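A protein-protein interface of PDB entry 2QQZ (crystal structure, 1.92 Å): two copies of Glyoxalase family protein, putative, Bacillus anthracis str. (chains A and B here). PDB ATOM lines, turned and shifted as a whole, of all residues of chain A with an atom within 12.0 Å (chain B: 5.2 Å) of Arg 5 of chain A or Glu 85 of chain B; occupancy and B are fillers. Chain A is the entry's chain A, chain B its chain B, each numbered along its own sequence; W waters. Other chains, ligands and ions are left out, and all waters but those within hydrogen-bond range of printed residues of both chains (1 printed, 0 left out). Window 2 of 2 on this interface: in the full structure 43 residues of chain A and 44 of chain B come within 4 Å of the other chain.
The side-chain carboxylate (OE2) of Glu 85 of chain B lies within salt-bridge range of the guanidinium group (NH1) of Arg 5 of chain A, at 3.0 Å.
OD1 of Asn 6 of chain A sits close to O of Gly 35 of chain B (3.5 Å).
OH of Tyr 7 of chain A sits at hydrogen-bond distance from OE2 of Glu 85 of chain B, 2.8 Å away.
The backbone carbonyl oxygen (O) of Tyr 7 of chain A sits at hydrogen-bond distance from the side-chain amide nitrogen (NE2) of Gln 9 of chain A (3.4 Å).
The side-chain carboxylate (OE1) of Glu 85 of chain B lies within salt-bridge range of the side-chain amino group (NZ) of Lys 82 of chain B, 3.3 Å away.
Glu 89 of chain B touches Met 4 of chain A (CB to SD, 3.7 Å).
CD1 of Phe 86 of chain B touches CD2 of Tyr 7 of chain A (3.5 Å).
Tyr 7 of chain A touches Glu 89 of chain B (OH to CG, 3.7 Å).
Of the printed residues of chain B, Arg 5 of chain A touches Glu 85.
Printed residues of chain A within 4 Å of Glu 85 of chain B: Arg 5 (3.0 Å) and Tyr 7 (2.8 Å).
No residue of chain A comes within 4 Å of Lys 82 of chain B.
No residue of chain A comes within 4 Å of Ile 83 of chain B.
Of the printed residues of chain A, Gly 35 of chain B touches Asn 6.
Of the printed residues of chain B, Tyr 7 of chain A touches Glu 85, Phe 86 and Glu 89.
Of the printed residues of chain A, Glu 89 of chain B touches Met 4 and Tyr 7.
Of the printed residues of chain B, Met 4 of chain A touches Glu 89 (3.7 Å).
Printed residues of chain B within 4 Å of Asn 6 of chain A: Gly 35.
Gln 9 of chain A touches none of the printed residues of chain B.
The nearest printed residue of chain A that does not touch Glu 85 of chain B is Met 4 of chain A (6.7 Å).
Of the 7 printed residues of chain A, 4 touch a printed residue of chain B.
Of the 9 printed residues of chain B, 4 touch a printed residue of chain A.
Among the printed residues, 6 pairs touch across the chains.
No position is printed for both chains.
Water W1 lies within hydrogen-bond range of the backbone carbonyl oxygen of Gly 35 of chain B (3.0 Å) and the side-chain amide oxygen of Asn 6 of chain A (3.0 Å).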
ATOM      1  N   MET A   4       9.295   8.561 -15.882  1.00  0.00           N
ATOM      2  CA  MET A   4       9.551  10.004 -16.151  1.00  0.00           C
ATOM      3  C   MET A   4      10.235  10.693 -14.978  1.00  0.00           C
ATOM      4  O   MET A   4       9.845  10.511 -13.816  1.00  0.00           O
ATOM      5  CB  MET A   4       8.244  10.730 -16.488  1.00  0.00           C
ATOM      6  CG  MET A   4       8.366  12.243 -16.617  1.00  0.00           C
ATOM      7  SD  MET A   4       7.893  12.898 -18.397  1.00  0.00           S
ATOM      8  CE  MET A   4       7.223  11.203 -19.207  1.00  0.00           C
ATOM      9  N   ARG A   5      11.252  11.493 -15.293  1.00  0.00           N
ATOM     10  CA  ARG A   5      11.987  12.241 -14.265  1.00  0.00           C
ATOM     11  C   ARG A   5      11.058  13.272 -13.622  1.00  0.00           C
ATOM     12  O   ARG A   5       9.919  13.472 -14.075  1.00  0.00           O
ATOM     13  CB  ARG A   5      13.254  12.891 -14.849  1.00  0.00           C
ATOM     14  CG  ARG A   5      14.124  11.894 -15.577  1.00  0.00           C
ATOM     15  CD  ARG A   5      15.551  12.335 -15.816  1.00  0.00           C
ATOM     16  NE  ARG A   5      16.339  11.157 -16.246  1.00  0.00           N
ATOM     17  CZ  ARG A   5      16.912  11.023 -17.464  1.00  0.00           C
ATOM     18  NH1 ARG A   5      16.847  12.016 -18.396  1.00  0.00           N
ATOM     19  NH2 ARG A   5      17.599   9.908 -17.735  1.00  0.00           N
ATOM     20  N   ASN A   6      11.531  13.908 -12.554  1.00  0.00           N
ATOM     21  CA  ASN A   6      10.728  14.866 -11.817  1.00  0.00           C
ATOM     22  C   ASN A   6      11.205  16.296 -12.099  1.00  0.00           C
ATOM     23  O   ASN A   6      12.055  16.837 -11.399  1.00  0.00           O
ATOM     24  CB  ASN A   6      10.711  14.509 -10.324  1.00  0.00           C
ATOM     25  CG  ASN A   6       9.902  13.244 -10.035  1.00  0.00           C
ATOM     26  OD1 ASN A   6       8.777  13.091 -10.512  1.00  0.00           O
ATOM     27  ND2 ASN A   6      10.466  12.348  -9.248  1.00  0.00           N
ATOM     28  N   TYR A   7      10.646  16.873 -13.162  1.00  0.00           N
ATOM     29  CA  TYR A   7      11.037  18.165 -13.730  1.00  0.00           C
ATOM     30  C   TYR A   7      10.393  19.334 -13.002  1.00  0.00           C
ATOM     31  O   TYR A   7      11.011  20.391 -12.856  1.00  0.00           O
ATOM     32  CB  TYR A   7      10.587  18.262 -15.180  1.00  0.00           C
ATOM     33  CG  TYR A   7      11.204  17.225 -16.076  1.00  0.00           C
ATOM     34  CD1 TYR A   7      12.450  17.443 -16.669  1.00  0.00           C
ATOM     35  CD2 TYR A   7      10.535  16.033 -16.348  1.00  0.00           C
ATOM     36  CE1 TYR A   7      13.023  16.502 -17.497  1.00  0.00           C
ATOM     37  CE2 TYR A   7      11.096  15.075 -17.206  1.00  0.00           C
ATOM     38  CZ  TYR A   7      12.352  15.309 -17.765  1.00  0.00           C
ATOM     39  OH  TYR A   7      12.946  14.357 -18.594  1.00  0.00           O
ATOM     40  N   ILE A   8       9.166  19.146 -12.527  1.00  0.00           N
ATOM     41  CA  ILE A   8       8.426  20.248 -11.917  1.00  0.00           C
ATOM     42  C   ILE A   8       8.897  20.583 -10.492  1.00  0.00           C
ATOM     43  O   ILE A   8       8.913  19.717  -9.617  1.00  0.00           O
ATOM     44  CB  ILE A   8       6.855  20.024 -11.936  1.00  0.00           C
ATOM     45  CG1 ILE A   8       6.303  19.925 -13.379  1.00  0.00           C
ATOM     46  CG2 ILE A   8       6.189  21.165 -11.162  1.00  0.00           C
ATOM     47  CD1 ILE A   8       4.756  19.609 -13.493  1.00  0.00           C
ATOM     48  N   GLN A   9       9.275  21.837 -10.244  1.00  0.00           N
ATOM     49  CA  GLN A   9       9.891  22.211  -8.978  1.00  0.00           C
ATOM     50  C   GLN A   9       8.952  22.892  -7.976  1.00  0.00           C
ATOM     51  O   GLN A   9       9.225  22.912  -6.755  1.00  0.00           O
ATOM     52  CB  GLN A   9      11.082  23.099  -9.266  1.00  0.00           C
ATOM     53  CG  GLN A   9      12.221  22.344 -10.009  1.00  0.00           C
ATOM     54  CD  GLN A   9      12.695  21.062  -9.297  1.00  0.00           C
ATOM     55  OE1 GLN A   9      12.951  21.043  -8.092  1.00  0.00           O
ATOM     56  NE2 GLN A   9      12.825  19.993 -10.054  1.00  0.00           N
ATOM     57  N   GLY A  10       7.848  23.436  -8.472  1.00  0.00           N
ATOM     58  CA  GLY A  10       6.949  24.183  -7.620  1.00  0.00           C
ATOM     59  C   GLY A  10       6.149  25.168  -8.461  1.00  0.00           C
ATOM     60  O   GLY A  10       6.270  25.194  -9.688  1.00  0.00           O
ATOM     61  N   GLY B  35       3.835  14.148 -14.571  1.00  0.00           N
ATOM     62  CA  GLY B  35       4.664  13.467 -13.578  1.00  0.00           C
ATOM     63  C   GLY B  35       4.564  14.029 -12.169  1.00  0.00           C
ATOM     64  O   GLY B  35       5.514  13.907 -11.403  1.00  0.00           O
ATOM     65  N   LYS B  82      15.331  21.889 -16.448  1.00  0.00           N
ATOM     66  CA  LYS B  82      15.559  21.295 -17.774  1.00  0.00           C
ATOM     67  C   LYS B  82      14.354  21.407 -18.690  1.00  0.00           C
ATOM     68  O   LYS B  82      13.886  20.405 -19.242  1.00  0.00           O
ATOM     69  CB  LYS B  82      15.977  19.817 -17.667  1.00  0.00           C
ATOM     70  CG  LYS B  82      17.356  19.617 -17.219  1.00  0.00           C
ATOM     71  CD  LYS B  82      18.331  19.647 -18.318  1.00  0.00           C
ATOM     72  CE  LYS B  82      18.219  18.423 -19.116  1.00  0.00           C
ATOM     73  NZ  LYS B  82      19.526  18.209 -19.665  1.00  0.00           N
ATOM     74  N   ILE B  83      13.836  22.627 -18.839  1.00  0.00           N
ATOM     75  CA  ILE B  83      12.543  22.799 -19.513  1.00  0.00           C
ATOM     76  C   ILE B  83      12.477  22.166 -20.920  1.00  0.00           C
ATOM     77  O   ILE B  83      11.449  21.588 -21.281  1.00  0.00           O
ATOM     78  CB  ILE B  83      12.105  24.279 -19.534  1.00  0.00           C
ATOM     79  CG1 ILE B  83      10.608  24.386 -19.878  1.00  0.00           C
ATOM     80  CG2 ILE B  83      13.042  25.071 -20.488  1.00  0.00           C
ATOM     81  CD1 ILE B  83       9.925  25.615 -19.340  1.00  0.00           C
ATOM     82  N   ASP B  84      13.580  22.234 -21.679  1.00  0.00           N
ATOM     83  CA  ASP B  84      13.581  21.755 -23.073  1.00  0.00           C
ATOM     84  C   ASP B  84      13.452  20.217 -23.161  1.00  0.00           C
ATOM     85  O   ASP B  84      12.831  19.681 -24.076  1.00  0.00           O
ATOM     86  CB  ASP B  84      14.803  22.298 -23.831  1.00  0.00           C
ATOM     87  CG  ASP B  84      14.703  23.813 -24.124  1.00  0.00           C
ATOM     88  OD1 ASP B  84      13.622  24.295 -24.550  1.00  0.00           O
ATOM     89  OD2 ASP B  84      15.719  24.518 -23.931  1.00  0.00           O
ATOM     90  N   GLU B  85      14.022  19.526 -22.180  1.00  0.00           N
ATOM     91  CA  GLU B  85      13.873  18.081 -22.017  1.00  0.00           C
ATOM     92  C   GLU B  85      12.408  17.731 -21.605  1.00  0.00           C
ATOM     93  O   GLU B  85      11.785  16.853 -22.205  1.00  0.00           O
ATOM     94  CB  GLU B  85      14.871  17.578 -20.970  1.00  0.00           C
ATOM     95  CG  GLU B  85      14.884  16.063 -20.806  1.00  0.00           C
ATOM     96  CD  GLU B  85      15.973  15.545 -19.864  1.00  0.00           C
ATOM     97  OE1 GLU B  85      17.147  15.923 -20.036  1.00  0.00           O
ATOM     98  OE2 GLU B  85      15.646  14.729 -18.962  1.00  0.00           O
ATOM     99  N   PHE B  86      11.873  18.437 -20.604  1.00  0.00           N
ATOM    100  CA  PHE B  86      10.495  18.256 -20.178  1.00  0.00           C
ATOM    101  C   PHE B  86       9.492  18.458 -21.325  1.00  0.00           C
ATOM    102  O   PHE B  86       8.548  17.659 -21.522  1.00  0.00           O
ATOM    103  CB  PHE B  86      10.197  19.251 -19.073  1.00  0.00           C
ATOM    104  CG  PHE B  86       8.769  19.243 -18.609  1.00  0.00           C
ATOM    105  CD1 PHE B  86       8.216  18.089 -18.023  1.00  0.00           C
ATOM    106  CD2 PHE B  86       7.991  20.381 -18.708  1.00  0.00           C
ATOM    107  CE1 PHE B  86       6.907  18.064 -17.575  1.00  0.00           C
ATOM    108  CE2 PHE B  86       6.646  20.364 -18.231  1.00  0.00           C
ATOM    109  CZ  PHE B  86       6.127  19.193 -17.666  1.00  0.00           C
ATOM    110  N   LYS B  87       9.685  19.539 -22.073  1.00  0.00           N
ATOM    111  CA  LYS B  87       8.807  19.843 -23.181  1.00  0.00           C
ATOM    112  C   LYS B  87       8.773  18.707 -24.205  1.00  0.00           C
ATOM    113  O   LYS B  87       7.699  18.341 -24.641  1.00  0.00           O
ATOM    114  CB  LYS B  87       9.203  21.142 -23.846  1.00  0.00           C
ATOM    115  CG  LYS B  87       8.190  21.539 -24.890  1.00  0.00           C
ATOM    116  CD  LYS B  87       8.429  22.912 -25.394  1.00  0.00           C
ATOM    117  CE  LYS B  87       9.516  22.879 -26.415  1.00  0.00           C
ATOM    118  NZ  LYS B  87       9.627  24.191 -27.103  1.00  0.00           N
ATOM    119  N   GLN B  88       9.934  18.153 -24.584  1.00  0.00           N
ATOM    120  CA  GLN B  88       9.985  17.038 -25.553  1.00  0.00           C
ATOM    121  C   GLN B  88       9.312  15.795 -25.007  1.00  0.00           C
ATOM    122  O   GLN B  88       8.685  15.058 -25.752  1.00  0.00           O
ATOM    123  CB  GLN B  88      11.426  16.714 -26.010  1.00  0.00           C
ATOM    124  CG  GLN B  88      12.104  17.865 -26.772  1.00  0.00           C
ATOM    125  CD  GLN B  88      11.287  18.379 -27.974  1.00  0.00           C
ATOM    126  OE1 GLN B  88      10.778  17.586 -28.780  1.00  0.00           O
ATOM    127  NE2 GLN B  88      11.173  19.716 -28.102  1.00  0.00           N
ATOM    128  N   GLU B  89       9.429  15.565 -23.707  1.00  0.00           N
ATOM    129  CA  GLU B  89       8.705  14.475 -23.066  1.00  0.00           C
ATOM    130  C   GLU B  89       7.194  14.650 -23.223  1.00  0.00           C
ATOM    131  O   GLU B  89       6.495  13.674 -23.408  1.00  0.00           O
ATOM    132  CB  GLU B  89       9.098  14.322 -21.595  1.00  0.00           C
ATOM    133  CG  GLU B  89      10.560  14.048 -21.358  1.00  0.00           C
ATOM    134  CD  GLU B  89      11.104  12.858 -22.178  1.00  0.00           C
ATOM    135  OE1 GLU B  89      10.498  11.751 -22.089  1.00  0.00           O
ATOM    136  OE2 GLU B  89      12.145  13.023 -22.897  1.00  0.00           O
HETATM  137  O   HOH W   1       6.280  12.005  -9.176  1.00  0.00           O
